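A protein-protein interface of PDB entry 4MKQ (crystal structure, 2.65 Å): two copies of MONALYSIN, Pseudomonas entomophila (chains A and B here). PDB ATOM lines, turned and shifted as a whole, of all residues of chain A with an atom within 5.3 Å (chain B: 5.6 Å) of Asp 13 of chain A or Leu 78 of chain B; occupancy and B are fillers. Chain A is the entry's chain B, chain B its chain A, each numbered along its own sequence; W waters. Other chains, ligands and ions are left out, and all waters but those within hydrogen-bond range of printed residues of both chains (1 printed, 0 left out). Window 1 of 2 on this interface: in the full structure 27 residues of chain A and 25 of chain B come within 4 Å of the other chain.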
ATOM      1  N   LYS A  11       6.780 -17.405 -20.543  1.00  0.00           N
ATOM      2  CA  LYS A  11       5.923 -17.633 -19.382  1.00  0.00           C
ATOM      3  C   LYS A  11       4.473 -17.364 -19.781  1.00  0.00           C
ATOM      4  O   LYS A  11       4.175 -16.292 -20.301  1.00  0.00           O
ATOM      5  CB  LYS A  11       6.368 -16.707 -18.231  1.00  0.00           C
ATOM      6  CG  LYS A  11       5.785 -17.039 -16.863  1.00  0.00           C
ATOM      7  CD  LYS A  11       6.303 -16.075 -15.811  1.00  0.00           C
ATOM      8  CE  LYS A  11       5.881 -16.466 -14.417  1.00  0.00           C
ATOM      9  NZ  LYS A  11       6.287 -15.444 -13.419  1.00  0.00           N
ATOM     10  N   GLY A  12       3.600 -18.345 -19.551  1.00  0.00           N
ATOM     11  CA  GLY A  12       2.182 -18.254 -19.884  1.00  0.00           C
ATOM     12  C   GLY A  12       1.849 -18.904 -21.210  1.00  0.00           C
ATOM     13  O   GLY A  12       2.561 -18.701 -22.197  1.00  0.00           O
ATOM     14  N   ASP A  13       0.748 -19.684 -21.232  1.00  0.00           N
ATOM     15  CA  ASP A  13       0.253 -20.464 -22.371  1.00  0.00           C
ATOM     16  C   ASP A  13       0.298 -19.744 -23.714  1.00  0.00           C
ATOM     17  O   ASP A  13       0.907 -20.257 -24.657  1.00  0.00           O
ATOM     18  CB  ASP A  13      -1.171 -20.987 -22.099  1.00  0.00           C
ATOM     19  CG  ASP A  13      -1.300 -21.877 -20.877  1.00  0.00           C
ATOM     20  OD1 ASP A  13      -0.391 -22.711 -20.645  1.00  0.00           O
ATOM     21  OD2 ASP A  13      -2.325 -21.763 -20.168  1.00  0.00           O
ATOM     22  N   PHE A  14      -0.323 -18.557 -23.793  1.00  0.00           N
ATOM     23  CA  PHE A  14      -0.400 -17.764 -25.018  1.00  0.00           C
ATOM     24  C   PHE A  14       0.944 -17.194 -25.458  1.00  0.00           C
ATOM     25  O   PHE A  14       1.136 -17.008 -26.657  1.00  0.00           O
ATOM     26  CB  PHE A  14      -1.470 -16.668 -24.896  1.00  0.00           C
ATOM     27  CG  PHE A  14      -2.891 -17.101 -25.195  1.00  0.00           C
ATOM     28  CD1 PHE A  14      -3.434 -18.232 -24.593  1.00  0.00           C
ATOM     29  CD2 PHE A  14      -3.701 -16.347 -26.034  1.00  0.00           C
ATOM     30  CE1 PHE A  14      -4.746 -18.624 -24.864  1.00  0.00           C
ATOM     31  CE2 PHE A  14      -5.019 -16.732 -26.290  1.00  0.00           C
ATOM     32  CZ  PHE A  14      -5.532 -17.870 -25.707  1.00  0.00           C
ATOM     33  N   ALA A  15       1.876 -16.943 -24.513  1.00  0.00           N
ATOM     34  CA  ALA A  15       3.220 -16.438 -24.831  1.00  0.00           C
ATOM     35  C   ALA A  15       4.070 -17.542 -25.450  1.00  0.00           C
ATOM     36  O   ALA A  15       4.783 -17.287 -26.419  1.00  0.00           O
ATOM     37  CB  ALA A  15       3.895 -15.878 -23.591  1.00  0.00           C
ATOM     38  N   ILE A  16       3.958 -18.777 -24.916  1.00  0.00           N
ATOM     39  CA  ILE A  16       4.652 -19.972 -25.401  1.00  0.00           C
ATOM     40  C   ILE A  16       4.152 -20.304 -26.819  1.00  0.00           C
ATOM     41  O   ILE A  16       4.966 -20.446 -27.735  1.00  0.00           O
ATOM     42  CB  ILE A  16       4.472 -21.162 -24.406  1.00  0.00           C
ATOM     43  CG1 ILE A  16       5.155 -20.871 -23.053  1.00  0.00           C
ATOM     44  CG2 ILE A  16       4.966 -22.485 -25.007  1.00  0.00           C
ATOM     45  CD1 ILE A  16       4.469 -21.486 -21.865  1.00  0.00           C
ATOM     46  N   ASP A  17       2.817 -20.390 -26.994  1.00  0.00           N
ATOM     47  CA  ASP A  17       2.179 -20.675 -28.277  1.00  0.00           C
ATOM     48  C   ASP A  17       2.444 -19.558 -29.287  1.00  0.00           C
ATOM     49  O   ASP A  17       2.795 -19.848 -30.430  1.00  0.00           O
ATOM     50  CB  ASP A  17       0.667 -20.900 -28.104  1.00  0.00           C
ATOM     51  CG  ASP A  17       0.258 -22.068 -27.214  1.00  0.00           C
ATOM     52  OD1 ASP A  17       1.100 -22.976 -26.988  1.00  0.00           O
ATOM     53  OD2 ASP A  17      -0.907 -22.089 -26.761  1.00  0.00           O
ATOM     54  N   GLY A  18       2.315 -18.307 -28.842  1.00  0.00           N
ATOM     55  CA  GLY A  18       2.547 -17.120 -29.659  1.00  0.00           C
ATOM     56  C   GLY A  18       3.940 -17.037 -30.246  1.00  0.00           C
ATOM     57  O   GLY A  18       4.100 -16.658 -31.409  1.00  0.00           O
ATOM     58  N   GLN A 117       0.078 -30.533 -27.170  1.00  0.00           N
ATOM     59  CA  GLN A 117      -1.019 -29.571 -27.049  1.00  0.00           C
ATOM     60  C   GLN A 117      -1.885 -29.618 -28.323  1.00  0.00           C
ATOM     61  O   GLN A 117      -1.423 -30.110 -29.358  1.00  0.00           O
ATOM     62  CB  GLN A 117      -0.479 -28.148 -26.779  1.00  0.00           C
ATOM     63  CG  GLN A 117       0.480 -28.024 -25.591  1.00  0.00           C
ATOM     64  CD  GLN A 117      -0.230 -27.994 -24.262  1.00  0.00           C
ATOM     65  OE1 GLN A 117      -0.576 -29.034 -23.689  1.00  0.00           O
ATOM     66  NE2 GLN A 117      -0.441 -26.797 -23.732  1.00  0.00           N
ATOM     67  N   ASP B  13      -0.965 -26.680 -14.416  1.00  0.00           N
ATOM     68  CA  ASP B  13      -1.568 -27.659 -15.331  1.00  0.00           C
ATOM     69  C   ASP B  13      -1.984 -28.976 -14.683  1.00  0.00           C
ATOM     70  O   ASP B  13      -3.149 -29.364 -14.793  1.00  0.00           O
ATOM     71  CB  ASP B  13      -0.644 -27.934 -16.531  1.00  0.00           C
ATOM     72  CG  ASP B  13      -0.292 -26.713 -17.358  1.00  0.00           C
ATOM     73  OD1 ASP B  13      -1.186 -25.869 -17.586  1.00  0.00           O
ATOM     74  OD2 ASP B  13       0.867 -26.624 -17.818  1.00  0.00           O
ATOM     75  N   ILE B  16      -4.808 -28.597 -11.922  1.00  0.00           N
ATOM     76  CA  ILE B  16      -6.100 -28.365 -12.573  1.00  0.00           C
ATOM     77  C   ILE B  16      -6.639 -29.700 -13.107  1.00  0.00           C
ATOM     78  O   ILE B  16      -7.774 -30.062 -12.789  1.00  0.00           O
ATOM     79  CB  ILE B  16      -5.977 -27.277 -13.680  1.00  0.00           C
ATOM     80  CG1 ILE B  16      -5.620 -25.892 -13.078  1.00  0.00           C
ATOM     81  CG2 ILE B  16      -7.244 -27.200 -14.545  1.00  0.00           C
ATOM     82  CD1 ILE B  16      -4.779 -25.027 -13.966  1.00  0.00           C
ATOM     83  N   VAL B  32      -9.104 -20.713 -11.769  1.00  0.00           N
ATOM     84  CA  VAL B  32      -7.688 -20.877 -12.106  1.00  0.00           C
ATOM     85  C   VAL B  32      -6.890 -19.614 -11.809  1.00  0.00           C
ATOM     86  O   VAL B  32      -7.234 -18.537 -12.300  1.00  0.00           O
ATOM     87  CB  VAL B  32      -7.478 -21.380 -13.571  1.00  0.00           C
ATOM     88  CG1 VAL B  32      -5.998 -21.454 -13.939  1.00  0.00           C
ATOM     89  CG2 VAL B  32      -8.146 -22.734 -13.797  1.00  0.00           C
ATOM     90  N   VAL B  37      -0.372 -12.537 -19.800  1.00  0.00           N
ATOM     91  CA  VAL B  37       0.535 -12.362 -20.935  1.00  0.00           C
ATOM     92  C   VAL B  37       0.027 -11.212 -21.803  1.00  0.00           C
ATOM     93  O   VAL B  37      -1.104 -10.772 -21.613  1.00  0.00           O
ATOM     94  CB  VAL B  37       0.751 -13.670 -21.755  1.00  0.00           C
ATOM     95  CG1 VAL B  37       1.402 -14.751 -20.909  1.00  0.00           C
ATOM     96  CG2 VAL B  37      -0.546 -14.174 -22.378  1.00  0.00           C
ATOM     97  N   PRO B  54      -5.481 -17.345 -17.737  1.00  0.00           N
ATOM     98  CA  PRO B  54      -6.505 -18.367 -17.452  1.00  0.00           C
ATOM     99  C   PRO B  54      -7.296 -17.949 -16.210  1.00  0.00           C
ATOM    100  O   PRO B  54      -6.737 -17.317 -15.309  1.00  0.00           O
ATOM    101  CB  PRO B  54      -5.692 -19.642 -17.226  1.00  0.00           C
ATOM    102  CG  PRO B  54      -4.365 -19.178 -16.788  1.00  0.00           C
ATOM    103  CD  PRO B  54      -4.126 -17.821 -17.381  1.00  0.00           C
ATOM    104  N   PHE B  56     -10.644 -19.911 -15.295  1.00  0.00           N
ATOM    105  CA  PHE B  56     -11.507 -21.020 -14.907  1.00  0.00           C
ATOM    106  C   PHE B  56     -11.216 -22.241 -15.769  1.00  0.00           C
ATOM    107  O   PHE B  56     -10.614 -22.122 -16.832  1.00  0.00           O
ATOM    108  CB  PHE B  56     -12.986 -20.585 -15.065  1.00  0.00           C
ATOM    109  CG  PHE B  56     -13.996 -21.417 -14.309  1.00  0.00           C
ATOM    110  CD1 PHE B  56     -14.215 -21.212 -12.950  1.00  0.00           C
ATOM    111  CD2 PHE B  56     -14.753 -22.383 -14.963  1.00  0.00           C
ATOM    112  CE1 PHE B  56     -15.135 -21.992 -12.252  1.00  0.00           C
ATOM    113  CE2 PHE B  56     -15.682 -23.158 -14.263  1.00  0.00           C
ATOM    114  CZ  PHE B  56     -15.861 -22.962 -12.914  1.00  0.00           C
ATOM    115  N   ALA B  57     -11.620 -23.417 -15.295  1.00  0.00           N
ATOM    116  CA  ALA B  57     -11.474 -24.682 -16.007  1.00  0.00           C
ATOM    117  C   ALA B  57     -12.660 -25.561 -15.663  1.00  0.00           C
ATOM    118  O   ALA B  57     -13.067 -25.604 -14.500  1.00  0.00           O
ATOM    119  CB  ALA B  57     -10.175 -25.364 -15.620  1.00  0.00           C
ATOM    120  N   TYR B  58     -13.250 -26.226 -16.672  1.00  0.00           N
ATOM    121  CA  TYR B  58     -14.412 -27.080 -16.440  1.00  0.00           C
ATOM    122  C   TYR B  58     -14.395 -28.370 -17.257  1.00  0.00           C
ATOM    123  O   TYR B  58     -13.753 -28.423 -18.307  1.00  0.00           O
ATOM    124  CB  TYR B  58     -15.732 -26.299 -16.639  1.00  0.00           C
ATOM    125  CG  TYR B  58     -16.046 -25.885 -18.062  1.00  0.00           C
ATOM    126  CD1 TYR B  58     -15.561 -24.691 -18.585  1.00  0.00           C
ATOM    127  CD2 TYR B  58     -16.907 -26.641 -18.855  1.00  0.00           C
ATOM    128  CE1 TYR B  58     -15.881 -24.284 -19.880  1.00  0.00           C
ATOM    129  CE2 TYR B  58     -17.229 -26.248 -20.152  1.00  0.00           C
ATOM    130  CZ  TYR B  58     -16.715 -25.066 -20.660  1.00  0.00           C
ATOM    131  OH  TYR B  58     -17.030 -24.673 -21.939  1.00  0.00           O
ATOM    132  N   VAL B  76     -10.977 -31.509 -20.299  1.00  0.00           N
ATOM    133  CA  VAL B  76     -10.894 -30.224 -19.597  1.00  0.00           C
ATOM    134  C   VAL B  76     -10.940 -29.070 -20.596  1.00  0.00           C
ATOM    135  O   VAL B  76     -10.173 -29.054 -21.561  1.00  0.00           O
ATOM    136  CB  VAL B  76      -9.667 -30.127 -18.638  1.00  0.00           C
ATOM    137  CG1 VAL B  76      -9.436 -28.696 -18.146  1.00  0.00           C
ATOM    138  CG2 VAL B  76      -9.824 -31.067 -17.453  1.00  0.00           C
ATOM    139  N   VAL B  77     -11.838 -28.109 -20.356  1.00  0.00           N
ATOM    140  CA  VAL B  77     -11.931 -26.884 -21.146  1.00  0.00           C
ATOM    141  C   VAL B  77     -11.308 -25.785 -20.282  1.00  0.00           C
ATOM    142  O   VAL B  77     -11.788 -25.528 -19.177  1.00  0.00           O
ATOM    143  CB  VAL B  77     -13.369 -26.529 -21.593  1.00  0.00           C
ATOM    144  CG1 VAL B  77     -13.370 -25.294 -22.480  1.00  0.00           C
ATOM    145  CG2 VAL B  77     -14.019 -27.689 -22.321  1.00  0.00           C
ATOM    146  N   LEU B  78     -10.206 -25.195 -20.757  1.00  0.00           N
ATOM    147  CA  LEU B  78      -9.505 -24.126 -20.059  1.00  0.00           C
ATOM    148  C   LEU B  78     -10.027 -22.780 -20.545  1.00  0.00           C
ATOM    149  O   LEU B  78      -9.980 -22.482 -21.739  1.00  0.00           O
ATOM    150  CB  LEU B  78      -7.982 -24.263 -20.239  1.00  0.00           C
ATOM    151  CG  LEU B  78      -7.063 -23.377 -19.375  1.00  0.00           C
ATOM    152  CD1 LEU B  78      -7.369 -23.510 -17.881  1.00  0.00           C
ATOM    153  CD2 LEU B  78      -5.610 -23.727 -19.616  1.00  0.00           C
ATOM    154  N   VAL B  79     -10.587 -21.999 -19.615  1.00  0.00           N
ATOM    155  CA  VAL B  79     -11.190 -20.695 -19.885  1.00  0.00           C
ATOM    156  C   VAL B  79     -10.192 -19.574 -19.596  1.00  0.00           C
ATOM    157  O   VAL B  79      -9.650 -19.481 -18.489  1.00  0.00           O
ATOM    158  CB  VAL B  79     -12.535 -20.505 -19.127  1.00  0.00           C
ATOM    159  CG1 VAL B  79     -13.240 -19.222 -19.553  1.00  0.00           C
ATOM    160  CG2 VAL B  79     -13.455 -21.705 -19.324  1.00  0.00           C
ATOM    161  N   TYR B  80      -9.963 -18.727 -20.609  1.00  0.00           N
ATOM    162  CA  TYR B  80      -9.073 -17.571 -20.564  1.00  0.00           C
ATOM    163  C   TYR B  80      -9.887 -16.297 -20.572  1.00  0.00           C
ATOM    164  O   TYR B  80     -10.957 -16.263 -21.175  1.00  0.00           O
ATOM    165  CB  TYR B  80      -8.142 -17.560 -21.789  1.00  0.00           C
ATOM    166  CG  TYR B  80      -7.165 -18.711 -21.843  1.00  0.00           C
ATOM    167  CD1 TYR B  80      -5.913 -18.615 -21.244  1.00  0.00           C
ATOM    168  CD2 TYR B  80      -7.468 -19.874 -22.543  1.00  0.00           C
ATOM    169  CE1 TYR B  80      -5.000 -19.667 -21.305  1.00  0.00           C
ATOM    170  CE2 TYR B  80      -6.565 -20.935 -22.606  1.00  0.00           C
ATOM    171  CZ  TYR B  80      -5.332 -20.827 -21.986  1.00  0.00           C
ATOM    172  OH  TYR B  80      -4.435 -21.863 -22.064  1.00  0.00           O
ATOM    173  N   SER B 113     -12.481 -16.715 -23.690  1.00  0.00           N
ATOM    174  CA  SER B 113     -12.258 -17.721 -24.730  1.00  0.00           C
ATOM    175  C   SER B 113     -12.005 -19.077 -24.079  1.00  0.00           C
ATOM    176  O   SER B 113     -11.504 -19.140 -22.956  1.00  0.00           O
ATOM    177  CB  SER B 113     -11.114 -17.330 -25.662  1.00  0.00           C
ATOM    178  OG  SER B 113      -9.846 -17.682 -25.136  1.00  0.00           O
ATOM    179  N   ALA B 114     -12.371 -20.154 -24.777  1.00  0.00           N
ATOM    180  CA  ALA B 114     -12.221 -21.514 -24.281  1.00  0.00           C
ATOM    181  C   ALA B 114     -11.328 -22.363 -25.184  1.00  0.00           C
ATOM    182  O   ALA B 114     -11.468 -22.332 -26.408  1.00  0.00           O
ATOM    183  CB  ALA B 114     -13.589 -22.150 -24.132  1.00  0.00           C
ATOM    184  N   ILE B 115     -10.404 -23.111 -24.564  1.00  0.00           N
ATOM    185  CA  ILE B 115      -9.476 -24.018 -25.240  1.00  0.00           C
ATOM    186  C   ILE B 115      -9.645 -25.426 -24.661  1.00  0.00           C
ATOM    187  O   ILE B 115      -9.482 -25.626 -23.454  1.00  0.00           O
ATOM    188  CB  ILE B 115      -8.001 -23.500 -25.194  1.00  0.00           C
ATOM    189  CG1 ILE B 115      -7.815 -22.298 -26.155  1.00  0.00           C
ATOM    190  CG2 ILE B 115      -6.985 -24.625 -25.503  1.00  0.00           C
ATOM    191  CD1 ILE B 115      -6.399 -21.638 -26.198  1.00  0.00           C
ATOM    192  N   THR B 116      -9.973 -26.394 -25.527  1.00  0.00           N
ATOM    193  CA  THR B 116     -10.135 -27.792 -25.131  1.00  0.00           C
ATOM    194  C   THR B 116      -8.757 -28.451 -25.008  1.00  0.00           C
ATOM    195  O   THR B 116      -7.956 -28.388 -25.942  1.00  0.00           O
ATOM    196  CB  THR B 116     -11.091 -28.511 -26.091  1.00  0.00           C
ATOM    197  OG1 THR B 116     -12.358 -27.853 -26.050  1.00  0.00           O
ATOM    198  CG2 THR B 116     -11.282 -29.975 -25.745  1.00  0.00           C
ATOM    199  N   GLN B 117      -8.486 -29.064 -23.845  1.00  0.00           N
ATOM    200  CA  GLN B 117      -7.221 -29.749 -23.568  1.00  0.00           C
ATOM    201  C   GLN B 117      -7.269 -31.191 -24.110  1.00  0.00           C
ATOM    202  O   GLN B 117      -8.355 -31.698 -24.403  1.00  0.00           O
ATOM    203  CB  GLN B 117      -6.884 -29.719 -22.061  1.00  0.00           C
ATOM    204  CG  GLN B 117      -6.894 -28.334 -21.400  1.00  0.00           C
ATOM    205  CD  GLN B 117      -5.745 -27.446 -21.810  1.00  0.00           C
ATOM    206  OE1 GLN B 117      -5.782 -26.779 -22.849  1.00  0.00           O
ATOM    207  NE2 GLN B 117      -4.720 -27.381 -20.975  1.00  0.00           N
HETATM  208  O   HOH W   1      -0.356 -23.334 -18.050  1.00  0.00           O
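Among the printed residues, no Asp or Glu carboxylate lies within 4 Å of a Lys or Arg side-chain nitrogen of the other chain.
Water W1 lies within hydrogen-bond range of OD1 of Asp 13 of chain A (2.7 Å) and OD1 of Asp 13 of chain B (2.7 Å).
Among the printed residues, merely in contact across the chains: Lys 11 of chain A with Val 37 of chain B (3.2 Å), Gly 12 of chain A with Val 37 of chain B (3.7 Å), Asp 13 of chain A with Leu 78 of chain B (3.9 Å), Phe 14 of chain A with Val 37 of chain B (3.7 Å), Phe 14 of chain A with Tyr 80 of chain B (3.7 Å), Phe 14 of chain A with Ile 115 of chain B (3.7 Å) and Ala 15 of chain A with Val 37 of chain B (3.8 Å).
The backbone NH (N) of Tyr 80 of chain B lies within hydrogen-bond range of the backbone carbonyl oxygen (O) of Ser 113 of chain B (2.8 Å). The backbone NH (N) of Leu 78 of chain B is in hydrogen-bond range of the backbone carbonyl oxygen (O) of Ile 115 of chain B, 2.8 Å away.
Asp 13 of chain A touches just these residues of chain B: Leu 78 and Tyr 80. Leu 78 of chain B touches just one residue of chain A: Asp 13 (3.9 Å). Of the printed residues of chain B, Gly 12 of chain A touches Val 37. Of the printed residues of chain B, Phe 14 of chain A touches Val 37, Tyr 80 and Ile 115. Ile 16 of chain A touches none of the printed residues of chain B. The nearest residue of chain B that does not touch Asp 13 of chain A is Asp 13 of chain B (4.5 Å). The nearest printed residue of chain A that does not touch Leu 78 of chain B is Phe 14 of chain A (7.2 Å).
The side-chain carboxylate (OD2) of Asp 13 of chain A sits at hydrogen-bond distance from the side-chain hydroxyl (OH) of Tyr 80 of chain B.
Positions printed for both chains: 13, 16 and 117. Of the 8 pairs that touch across the chains among the printed residues, none has its exchanged pair printed and touching as well.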
